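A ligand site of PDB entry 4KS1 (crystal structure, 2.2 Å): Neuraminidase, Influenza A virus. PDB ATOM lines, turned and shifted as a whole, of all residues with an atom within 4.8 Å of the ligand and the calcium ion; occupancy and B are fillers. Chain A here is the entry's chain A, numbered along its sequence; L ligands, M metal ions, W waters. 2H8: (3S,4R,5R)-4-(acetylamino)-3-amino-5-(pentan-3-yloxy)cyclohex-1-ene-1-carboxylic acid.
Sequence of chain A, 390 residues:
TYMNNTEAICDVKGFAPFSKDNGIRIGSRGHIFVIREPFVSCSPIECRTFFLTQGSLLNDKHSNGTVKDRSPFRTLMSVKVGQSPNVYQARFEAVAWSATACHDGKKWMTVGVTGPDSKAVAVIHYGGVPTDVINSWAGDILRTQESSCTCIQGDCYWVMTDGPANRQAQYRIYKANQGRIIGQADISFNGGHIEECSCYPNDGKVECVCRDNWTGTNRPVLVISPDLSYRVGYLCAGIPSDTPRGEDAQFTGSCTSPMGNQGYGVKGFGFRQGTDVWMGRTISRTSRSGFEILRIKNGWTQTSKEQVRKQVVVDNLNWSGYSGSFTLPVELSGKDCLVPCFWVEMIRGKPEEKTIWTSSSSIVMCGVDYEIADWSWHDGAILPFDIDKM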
ATOM      1  N   ARG A  36       3.542   2.691   6.948  1.00  0.00           N
ATOM      2  CA  ARG A  36       4.334   3.015   8.115  1.00  0.00           C
ATOM      3  C   ARG A  36       3.567   4.069   8.883  1.00  0.00           C
ATOM      4  O   ARG A  36       2.456   4.453   8.487  1.00  0.00           O
ATOM      5  CB  ARG A  36       5.734   3.509   7.756  1.00  0.00           C
ATOM      6  CG  ARG A  36       6.803   2.430   7.898  1.00  0.00           C
ATOM      7  CD  ARG A  36       8.123   3.012   8.347  1.00  0.00           C
ATOM      8  NE  ARG A  36       7.999   3.661   9.647  1.00  0.00           N
ATOM      9  CZ  ARG A  36       8.815   4.605  10.097  1.00  0.00           C
ATOM     10  NH1 ARG A  36       8.601   5.124  11.301  1.00  0.00           N
ATOM     11  NH2 ARG A  36       9.822   5.043   9.357  1.00  0.00           N
ATOM     12  N   GLU A  37       4.152   4.541   9.979  1.00  0.00           N
ATOM     13  CA  GLU A  37       3.519   5.535  10.847  1.00  0.00           C
ATOM     14  C   GLU A  37       2.079   5.214  11.260  1.00  0.00           C
ATOM     15  O   GLU A  37       1.184   6.026  11.064  1.00  0.00           O
ATOM     16  CB  GLU A  37       3.560   6.921  10.189  1.00  0.00           C
ATOM     17  CG  GLU A  37       4.985   7.440   9.936  1.00  0.00           C
ATOM     18  CD  GLU A  37       5.566   6.967   8.607  1.00  0.00           C
ATOM     19  OE1 GLU A  37       4.783   6.686   7.682  1.00  0.00           O
ATOM     20  OE2 GLU A  37       6.808   6.874   8.505  1.00  0.00           O
ATOM     21  N   ASP A  69       9.840   8.163   2.276  1.00  0.00           N
ATOM     22  CA  ASP A  69       8.867   8.806   3.149  1.00  0.00           C
ATOM     23  C   ASP A  69       7.685   9.483   2.443  1.00  0.00           C
ATOM     24  O   ASP A  69       6.555   9.413   2.924  1.00  0.00           O
ATOM     25  CB  ASP A  69       9.554   9.802   4.068  1.00  0.00           C
ATOM     26  CG  ASP A  69      10.360   9.121   5.153  1.00  0.00           C
ATOM     27  OD1 ASP A  69       9.784   8.251   5.859  1.00  0.00           O
ATOM     28  OD2 ASP A  69      11.563   9.429   5.278  1.00  0.00           O
ATOM     29  N   ARG A  70       7.931  10.156   1.323  1.00  0.00           N
ATOM     30  CA  ARG A  70       6.891  10.993   0.736  1.00  0.00           C
ATOM     31  C   ARG A  70       6.657  10.682  -0.747  1.00  0.00           C
ATOM     32  O   ARG A  70       7.602  10.522  -1.513  1.00  0.00           O
ATOM     33  CB  ARG A  70       7.200  12.475   0.962  1.00  0.00           C
ATOM     34  CG  ARG A  70       7.349  12.847   2.446  1.00  0.00           C
ATOM     35  CD  ARG A  70       7.684  14.325   2.691  1.00  0.00           C
ATOM     36  NE  ARG A  70       8.906  14.758   2.016  1.00  0.00           N
ATOM     37  CZ  ARG A  70      10.144  14.441   2.404  1.00  0.00           C
ATOM     38  NH1 ARG A  70      11.184  14.894   1.715  1.00  0.00           N
ATOM     39  NH2 ARG A  70      10.337  13.667   3.460  1.00  0.00           N
ATOM     40  N   ARG A  74       0.703   8.182  -1.179  1.00  0.00           N
ATOM     41  CA  ARG A  74       0.492   7.879   0.238  1.00  0.00           C
ATOM     42  C   ARG A  74      -0.850   8.438   0.712  1.00  0.00           C
ATOM     43  O   ARG A  74      -1.192   9.573   0.403  1.00  0.00           O
ATOM     44  CB  ARG A  74       1.636   8.416   1.105  1.00  0.00           C
ATOM     45  CG  ARG A  74       2.990   7.829   0.771  1.00  0.00           C
ATOM     46  CD  ARG A  74       3.895   7.846   1.992  1.00  0.00           C
ATOM     47  NE  ARG A  74       3.542   6.815   2.957  1.00  0.00           N
ATOM     48  CZ  ARG A  74       4.256   6.530   4.047  1.00  0.00           C
ATOM     49  NH1 ARG A  74       3.873   5.573   4.884  1.00  0.00           N
ATOM     50  NH2 ARG A  74       5.376   7.203   4.296  1.00  0.00           N
ATOM     51  N   TRP A  97       1.140  12.074   3.458  1.00  0.00           N
ATOM     52  CA  TRP A  97       2.396  11.447   3.834  1.00  0.00           C
ATOM     53  C   TRP A  97       2.815  11.880   5.241  1.00  0.00           C
ATOM     54  O   TRP A  97       3.892  11.517   5.724  1.00  0.00           O
ATOM     55  CB  TRP A  97       3.523  11.695   2.819  1.00  0.00           C
ATOM     56  CG  TRP A  97       3.598  13.067   2.160  1.00  0.00           C
ATOM     57  CD1 TRP A  97       3.357  13.351   0.842  1.00  0.00           C
ATOM     58  CD2 TRP A  97       3.989  14.311   2.775  1.00  0.00           C
ATOM     59  NE1 TRP A  97       3.547  14.699   0.610  1.00  0.00           N
ATOM     60  CE2 TRP A  97       3.937  15.300   1.764  1.00  0.00           C
ATOM     61  CE3 TRP A  97       4.366  14.665   4.065  1.00  0.00           C
ATOM     62  CZ2 TRP A  97       4.252  16.631   2.024  1.00  0.00           C
ATOM     63  CZ3 TRP A  97       4.675  15.996   4.317  1.00  0.00           C
ATOM     64  CH2 TRP A  97       4.616  16.963   3.298  1.00  0.00           C
ATOM     65  N   SER A  98       1.932  12.639   5.897  1.00  0.00           N
ATOM     66  CA  SER A  98       2.028  12.957   7.321  1.00  0.00           C
ATOM     67  C   SER A  98       0.621  13.238   7.832  1.00  0.00           C
ATOM     68  O   SER A  98      -0.187  13.862   7.123  1.00  0.00           O
ATOM     69  CB  SER A  98       2.943  14.156   7.571  1.00  0.00           C
ATOM     70  OG  SER A  98       3.021  14.470   8.958  1.00  0.00           O
ATOM     71  N   ILE A 141       8.622  21.048   3.967  1.00  0.00           N
ATOM     72  CA  ILE A 141       7.941  19.858   4.465  1.00  0.00           C
ATOM     73  C   ILE A 141       7.080  20.131   5.680  1.00  0.00           C
ATOM     74  O   ILE A 141       7.399  19.708   6.790  1.00  0.00           O
ATOM     75  CB  ILE A 141       8.927  18.706   4.794  1.00  0.00           C
ATOM     76  CG1 ILE A 141      10.069  18.663   3.781  1.00  0.00           C
ATOM     77  CG2 ILE A 141       8.188  17.372   4.850  1.00  0.00           C
ATOM     78  CD1 ILE A 141      11.109  17.585   4.095  1.00  0.00           C
ATOM     79  N   ARG A 143       4.411  19.395   8.257  1.00  0.00           N
ATOM     80  CA  ARG A 143       4.259  18.046   8.810  1.00  0.00           C
ATOM     81  C   ARG A 143       3.697  18.059  10.227  1.00  0.00           C
ATOM     82  O   ARG A 143       3.691  19.098  10.901  1.00  0.00           O
ATOM     83  CB  ARG A 143       5.597  17.312   8.801  1.00  0.00           C
ATOM     84  CG  ARG A 143       6.708  18.040   9.580  1.00  0.00           C
ATOM     85  CD  ARG A 143       8.058  17.448   9.224  1.00  0.00           C
ATOM     86  NE  ARG A 143       9.194  18.039   9.935  1.00  0.00           N
ATOM     87  CZ  ARG A 143       9.906  19.068   9.476  1.00  0.00           C
ATOM     88  NH1 ARG A 143      10.945  19.514  10.172  1.00  0.00           N
ATOM     89  NH2 ARG A 143       9.592  19.646   8.324  1.00  0.00           N
ATOM     90  N   GLU A 146       1.816  12.287  13.567  1.00  0.00           N
ATOM     91  CA  GLU A 146       1.812  10.840  13.337  1.00  0.00           C
ATOM     92  C   GLU A 146       1.277  10.068  14.561  1.00  0.00           C
ATOM     93  O   GLU A 146       1.607   8.903  14.767  1.00  0.00           O
ATOM     94  CB  GLU A 146       3.171  10.286  12.900  1.00  0.00           C
ATOM     95  CG  GLU A 146       4.027  11.218  12.034  1.00  0.00           C
ATOM     96  CD  GLU A 146       3.448  11.481  10.645  1.00  0.00           C
ATOM     97  OE1 GLU A 146       2.312  11.027  10.345  1.00  0.00           O
ATOM     98  OE2 GLU A 146       4.140  12.152   9.840  1.00  0.00           O
ATOM     99  N   ALA A 165      14.812  19.476   9.236  1.00  0.00           N
ATOM    100  CA  ALA A 165      14.700  18.323  10.121  1.00  0.00           C
ATOM    101  C   ALA A 165      15.950  18.122  10.974  1.00  0.00           C
ATOM    102  O   ALA A 165      16.014  17.179  11.765  1.00  0.00           O
ATOM    103  CB  ALA A 165      14.416  17.075   9.327  1.00  0.00           C
ATOM    104  N   GLU A 195       9.476  17.655  16.771  1.00  0.00           N
ATOM    105  CA  GLU A 195       8.889  16.836  15.727  1.00  0.00           C
ATOM    106  C   GLU A 195       7.945  15.813  16.309  1.00  0.00           C
ATOM    107  O   GLU A 195       8.123  15.382  17.450  1.00  0.00           O
ATOM    108  CB  GLU A 195       9.969  16.067  14.963  1.00  0.00           C
ATOM    109  CG  GLU A 195      11.016  16.927  14.305  1.00  0.00           C
ATOM    110  CD  GLU A 195      10.636  17.348  12.903  1.00  0.00           C
ATOM    111  OE1 GLU A 195      11.534  17.772  12.145  1.00  0.00           O
ATOM    112  OE2 GLU A 195       9.433  17.262  12.553  1.00  0.00           O
ATOM    113  N   GLU A 196       6.938  15.431  15.540  1.00  0.00           N
ATOM    114  CA  GLU A 196       6.157  14.229  15.800  1.00  0.00           C
ATOM    115  C   GLU A 196       5.698  14.105  17.253  1.00  0.00           C
ATOM    116  O   GLU A 196       6.035  13.133  17.940  1.00  0.00           O
ATOM    117  CB  GLU A 196       6.984  13.004  15.388  1.00  0.00           C
ATOM    118  CG  GLU A 196       7.293  12.983  13.886  1.00  0.00           C
ATOM    119  CD  GLU A 196       8.275  11.906  13.506  1.00  0.00           C
ATOM    120  OE1 GLU A 196       9.058  11.470  14.371  1.00  0.00           O
ATOM    121  OE2 GLU A 196       8.274  11.471  12.337  1.00  0.00           O
ATOM    122  N   ARG A 211       9.797  14.824  19.647  1.00  0.00           N
ATOM    123  CA  ARG A 211      11.078  14.346  19.130  1.00  0.00           C
ATOM    124  C   ARG A 211      11.956  15.533  18.747  1.00  0.00           C
ATOM    125  O   ARG A 211      11.574  16.337  17.906  1.00  0.00           O
ATOM    126  CB  ARG A 211      10.848  13.439  17.920  1.00  0.00           C
ATOM    127  CG  ARG A 211      12.076  13.150  17.043  1.00  0.00           C
ATOM    128  CD  ARG A 211      11.673  12.323  15.812  1.00  0.00           C
ATOM    129  NE  ARG A 211      12.798  12.073  14.912  1.00  0.00           N
ATOM    130  CZ  ARG A 211      12.736  11.310  13.813  1.00  0.00           C
ATOM    131  NH1 ARG A 211      13.808  11.142  13.053  1.00  0.00           N
ATOM    132  NH2 ARG A 211      11.594  10.708  13.469  1.00  0.00           N
ATOM    133  N   ASP A 212      13.120  15.642  19.388  1.00  0.00           N
ATOM    134  CA  ASP A 212      14.138  16.582  18.963  1.00  0.00           C
ATOM    135  C   ASP A 212      15.023  15.853  17.956  1.00  0.00           C
ATOM    136  O   ASP A 212      15.734  14.921  18.303  1.00  0.00           O
ATOM    137  CB  ASP A 212      14.965  17.062  20.166  1.00  0.00           C
ATOM    138  CG  ASP A 212      16.032  18.100  19.792  1.00  0.00           C
ATOM    139  OD1 ASP A 212      16.095  19.150  20.453  1.00  0.00           O
ATOM    140  OD2 ASP A 212      16.822  17.859  18.855  1.00  0.00           O
ATOM    141  N   ASN A 213      14.973  16.290  16.696  1.00  0.00           N
ATOM    142  CA  ASN A 213      15.756  15.670  15.641  1.00  0.00           C
ATOM    143  C   ASN A 213      17.025  16.474  15.316  1.00  0.00           C
ATOM    144  O   ASN A 213      17.711  16.196  14.332  1.00  0.00           O
ATOM    145  CB  ASN A 213      14.898  15.471  14.384  1.00  0.00           C
ATOM    146  CG  ASN A 213      15.380  14.317  13.518  1.00  0.00           C
ATOM    147  OD1 ASN A 213      15.389  13.165  13.951  1.00  0.00           O
ATOM    148  ND2 ASN A 213      15.779  14.632  12.285  1.00  0.00           N
ATOM    149  N   GLY A 216      19.159  17.005  20.533  1.00  0.00           N
ATOM    150  CA  GLY A 216      18.733  16.428  21.800  1.00  0.00           C
ATOM    151  C   GLY A 216      18.456  14.937  21.799  1.00  0.00           C
ATOM    152  O   GLY A 216      17.858  14.398  20.862  1.00  0.00           O
ATOM    153  N   THR A 217      18.905  14.258  22.863  1.00  0.00           N
ATOM    154  CA  THR A 217      18.563  12.851  23.060  1.00  0.00           C
ATOM    155  C   THR A 217      17.527  12.724  24.181  1.00  0.00           C
ATOM    156  O   THR A 217      17.054  11.629  24.487  1.00  0.00           O
ATOM    157  CB  THR A 217      19.795  11.995  23.367  1.00  0.00           C
ATOM    158  OG1 THR A 217      20.349  12.402  24.636  1.00  0.00           O
ATOM    159  CG2 THR A 217      20.843  12.150  22.274  1.00  0.00           C
ATOM    160  N   ASP A 242      15.364   9.209  23.659  1.00  0.00           N
ATOM    161  CA  ASP A 242      15.324   9.264  22.192  1.00  0.00           C
ATOM    162  C   ASP A 242      16.246   8.183  21.621  1.00  0.00           C
ATOM    163  O   ASP A 242      16.938   7.496  22.367  1.00  0.00           O
ATOM    164  CB  ASP A 242      15.718  10.665  21.707  1.00  0.00           C
ATOM    165  CG  ASP A 242      15.255  10.963  20.268  1.00  0.00           C
ATOM    166  OD1 ASP A 242      15.504  12.097  19.817  1.00  0.00           O
ATOM    167  OD2 ASP A 242      14.652  10.091  19.598  1.00  0.00           O
ATOM    168  N   GLN A 262      23.490  14.698  19.995  1.00  0.00           N
ATOM    169  CA  GLN A 262      23.413  13.748  18.895  1.00  0.00           C
ATOM    170  C   GLN A 262      22.269  14.127  17.963  1.00  0.00           C
ATOM    171  O   GLN A 262      21.255  14.656  18.405  1.00  0.00           O
ATOM    172  CB  GLN A 262      23.189  12.324  19.403  1.00  0.00           C
ATOM    173  CG  GLN A 262      24.379  11.713  20.115  1.00  0.00           C
ATOM    174  CD  GLN A 262      24.208  10.235  20.359  1.00  0.00           C
ATOM    175  OE1 GLN A 262      24.148   9.785  21.502  1.00  0.00           O
ATOM    176  NE2 GLN A 262      24.154   9.464  19.279  1.00  0.00           N
ATOM    177  N   GLY A 263      22.440  13.839  16.677  1.00  0.00           N
ATOM    178  CA  GLY A 263      21.405  14.111  15.701  1.00  0.00           C
ATOM    179  C   GLY A 263      20.380  12.983  15.621  1.00  0.00           C
ATOM    180  O   GLY A 263      20.427  12.037  16.412  1.00  0.00           O
ATOM    181  N   TYR A 264      19.454  13.113  14.676  1.00  0.00           N
ATOM    182  CA  TYR A 264      18.397  12.121  14.445  1.00  0.00           C
ATOM    183  C   TYR A 264      17.503  11.920  15.672  1.00  0.00           C
ATOM    184  O   TYR A 264      17.535  12.702  16.618  1.00  0.00           O
ATOM    185  CB  TYR A 264      18.987  10.789  13.947  1.00  0.00           C
ATOM    186  CG  TYR A 264      18.041   9.960  13.082  1.00  0.00           C
ATOM    187  CD1 TYR A 264      17.262  10.558  12.090  1.00  0.00           C
ATOM    188  CD2 TYR A 264      17.959   8.583  13.235  1.00  0.00           C
ATOM    189  CE1 TYR A 264      16.414   9.793  11.277  1.00  0.00           C
ATOM    190  CE2 TYR A 264      17.112   7.815  12.447  1.00  0.00           C
ATOM    191  CZ  TYR A 264      16.349   8.422  11.468  1.00  0.00           C
ATOM    192  OH  TYR A 264      15.515   7.649  10.682  1.00  0.00           O
ATOM    193  N   GLY A 265      16.707  10.853  15.632  1.00  0.00           N
ATOM    194  CA  GLY A 265      15.754  10.574  16.680  1.00  0.00           C
ATOM    195  C   GLY A 265      14.724   9.557  16.241  1.00  0.00           C
ATOM    196  O   GLY A 265      14.872   8.915  15.197  1.00  0.00           O
ATOM    197  N   ARG A 288      16.655   0.929  16.189  1.00  0.00           N
ATOM    198  CA  ARG A 288      15.239   0.833  16.520  1.00  0.00           C
ATOM    199  C   ARG A 288      14.842  -0.614  16.833  1.00  0.00           C
ATOM    200  O   ARG A 288      14.022  -1.215  16.136  1.00  0.00           O
ATOM    201  CB  ARG A 288      14.390   1.443  15.405  1.00  0.00           C
ATOM    202  CG  ARG A 288      14.574   2.947  15.288  1.00  0.00           C
ATOM    203  CD  ARG A 288      14.098   3.503  13.957  1.00  0.00           C
ATOM    204  NE  ARG A 288      14.069   4.959  13.962  1.00  0.00           N
ATOM    205  CZ  ARG A 288      13.411   5.699  13.078  1.00  0.00           C
ATOM    206  NH1 ARG A 288      13.425   7.022  13.189  1.00  0.00           N
ATOM    207  NH2 ARG A 288      12.726   5.126  12.095  1.00  0.00           N
ATOM    208  N   TYR A 322       8.575   3.631  15.840  1.00  0.00           N
ATOM    209  CA  TYR A 322       7.801   4.685  16.463  1.00  0.00           C
ATOM    210  C   TYR A 322       6.957   4.195  17.643  1.00  0.00           C
ATOM    211  O   TYR A 322       6.725   3.003  17.807  1.00  0.00           O
ATOM    212  CB  TYR A 322       6.866   5.341  15.437  1.00  0.00           C
ATOM    213  CG  TYR A 322       7.526   6.378  14.555  1.00  0.00           C
ATOM    214  CD1 TYR A 322       8.912   6.454  14.433  1.00  0.00           C
ATOM    215  CD2 TYR A 322       6.761   7.306  13.851  1.00  0.00           C
ATOM    216  CE1 TYR A 322       9.509   7.411  13.636  1.00  0.00           C
ATOM    217  CE2 TYR A 322       7.351   8.267  13.059  1.00  0.00           C
ATOM    218  CZ  TYR A 322       8.721   8.308  12.948  1.00  0.00           C
ATOM    219  OH  TYR A 322       9.291   9.279  12.159  1.00  0.00           O
HETATM  220  CAA 2H8 L   1      12.114  14.059  11.625  1.00  0.00           C
HETATM  221  CAI 2H8 L   1      10.623  14.090  11.277  1.00  0.00           C
HETATM  222  CAR 2H8 L   1      10.381  14.166   9.711  1.00  0.00           C
HETATM  223  CAJ 2H8 L   1      10.989  15.462   9.054  1.00  0.00           C
HETATM  224  CAB 2H8 L   1      10.544  15.651   7.589  1.00  0.00           C
HETATM  225  OAM 2H8 L   1      10.896  13.002   9.032  1.00  0.00           O
HETATM  226  CAS 2H8 L   1      10.287  11.751   9.339  1.00  0.00           C
HETATM  227  CAK 2H8 L   1      11.419  10.735   9.584  1.00  0.00           C
HETATM  228  CAP 2H8 L   1      10.948   9.369   9.627  1.00  0.00           C
HETATM  229  CAO 2H8 L   1      11.662   8.463  10.433  1.00  0.00           C
HETATM  230  OAG 2H8 L   1      12.517   8.915  11.278  1.00  0.00           O
HETATM  231  OAF 2H8 L   1      11.423   7.215  10.315  1.00  0.00           O
HETATM  232  CAH 2H8 L   1       9.750   8.948   9.000  1.00  0.00           C
HETATM  233  CAQ 2H8 L   1       8.828   9.891   8.474  1.00  0.00           C
HETATM  234  NAD 2H8 L   1       8.004   9.324   7.394  1.00  0.00           N
HETATM  235  CAT 2H8 L   1       9.448  11.297   8.133  1.00  0.00           C
HETATM  236  NAL 2H8 L   1       8.382  12.258   7.914  1.00  0.00           N
HETATM  237  CAN 2H8 L   1       8.182  12.908   6.752  1.00  0.00           C
HETATM  238  OAE 2H8 L   1       8.862  12.782   5.771  1.00  0.00           O
HETATM  239  CAC 2H8 L   1       6.987  13.869   6.741  1.00  0.00           C
HETATM  240 CA    CA M   1      17.294  13.321  18.804  1.00  0.00          CA
HETATM  241  O   HOH W   1       6.387  10.283   5.341  1.00  0.00           O
HETATM  242  O   HOH W   2       7.717   6.480   5.858  1.00  0.00           O
HETATM  243  O   HOH W   3       5.517  10.207   8.172  1.00  0.00           O
HETATM  244  O   HOH W   4      19.068  11.622  18.709  1.00  0.00           O
HETATM  245  O   HOH W   5       6.887  12.513  10.324  1.00  0.00           O
HETATM  246  O   HOH W   6      11.890   7.193   7.511  1.00  0.00           O
HETATM  247  O   HOH W   7      13.493  12.911   7.857  1.00  0.00           O
HETATM  248  O   HOH W   8      18.978  14.945  17.719  1.00  0.00           O
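A nitrogen (NAD) of the ligand is in salt-bridge range of the side-chain carboxylate (OE2) of Glu 37, at 2.9 Å.
A nitrogen (NAD) of the ligand is in salt-bridge range of the side-chain carboxylate (OD1) of Asp 69 (2.6 Å).
The guanidinium group (NH2) of Arg 70 sits at hydrogen-bond distance from an oxygen (OAE) of the ligand, at 2.9 Å.
OAG of the ligand lies close to OH of Tyr 322.
The guanidinium group (NH1) of Arg 288 is in salt-bridge range of an oxygen (OAG) of the ligand (2.8 Å).
The guanidinium group of Arg 211 is in salt-bridge range of an oxygen (OAG) of the ligand (3.0 Å).
The guanidinium group (NH2) of Arg 36 is in salt-bridge range of an oxygen (OAF) of the ligand (2.9 Å).
An oxygen (OAG) of the ligand is in hydrogen-bond range of the side-chain hydroxyl (OH) of Tyr 264 (3.3 Å).
The guanidinium group of Arg 211 is in hydrogen-bond range of the backbone carbonyl oxygen of Gly 265, 3.3 Å away.
N of Asp 242 sits at hydrogen-bond distance from O of Thr 217 (3.1 Å).
The side-chain carboxylate of Glu 196 is in salt-bridge range of the guanidinium group of Arg 211 (2.8 Å).
OH of Tyr 322 is in hydrogen-bond range of OE2 of Glu 196, 2.4 Å away.
O of Arg 211 is in hydrogen-bond range of N of Glu 195 (2.7 Å).
NH1 of Arg 288 sits at hydrogen-bond distance from O of Gly 265, 3.1 Å away.
The backbone carbonyl oxygen (O) of Asp 69 lies within hydrogen-bond range of the guanidinium group (NH2) of Arg 74 (2.9 Å).
O of Tyr 264 sits close to OD1 of Asn 213.
Trp 97 touches the ligand (CE3 to CAC, 3.8 Å).
NE of Arg 143 touches CAJ of the ligand, at 3.3 Å.
Ala 165 touches the ligand (CB to CAJ, 3.8 Å).
Glu 195 touches the ligand.
Glu 196 touches the ligand (OE2 to CAS, 3.6 Å).
Asn 213 touches the ligand.
Hydrophobic or aromatic side chains within 4 Å of the ligand: Trp 97, Ala 165, Tyr 264 and Tyr 322.
Residues that only touch the calcium ion: Gly 265.
Of the 25 residues printed, 5 come within 4 Å of the calcium ion.
The calcium ion is bound by the backbone carbonyl oxygen of Tyr 264 (2.3 Å), the backbone carbonyl oxygen of Asp 212 (2.3 Å), the backbone carbonyl oxygen of Gly 216 (2.4 Å), the side-chain carboxylate of Asp 242 (2.4 Å), water W4 (2.5 Å) and water W8 (2.6 Å).
The calcium ion has six donor atoms within binding distance.
Water W3 lies within hydrogen-bond range of a nitrogen (NAD) of the ligand, the side-chain carboxylate of Glu 146 and the backbone carbonyl oxygen of Trp 97.
Water W1 lies within hydrogen-bond range of O of Asp 69 (2.6 Å), NAD of the ligand (2.8 Å), O of Trp 97 (2.8 Å) and NH2 of Arg 74 (3.4 Å).
Water W6 bridges OAF of the ligand and OD1 of Asp 69.
Water W5 lies within hydrogen-bond range of OE2 of Glu 196, OE2 of Glu 146 and NAL of the ligand.
Water W2 lies within hydrogen-bond range of OD1 of Asp 69, OE2 of Glu 37, NH2 of Arg 74 and NAD of the ligand.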
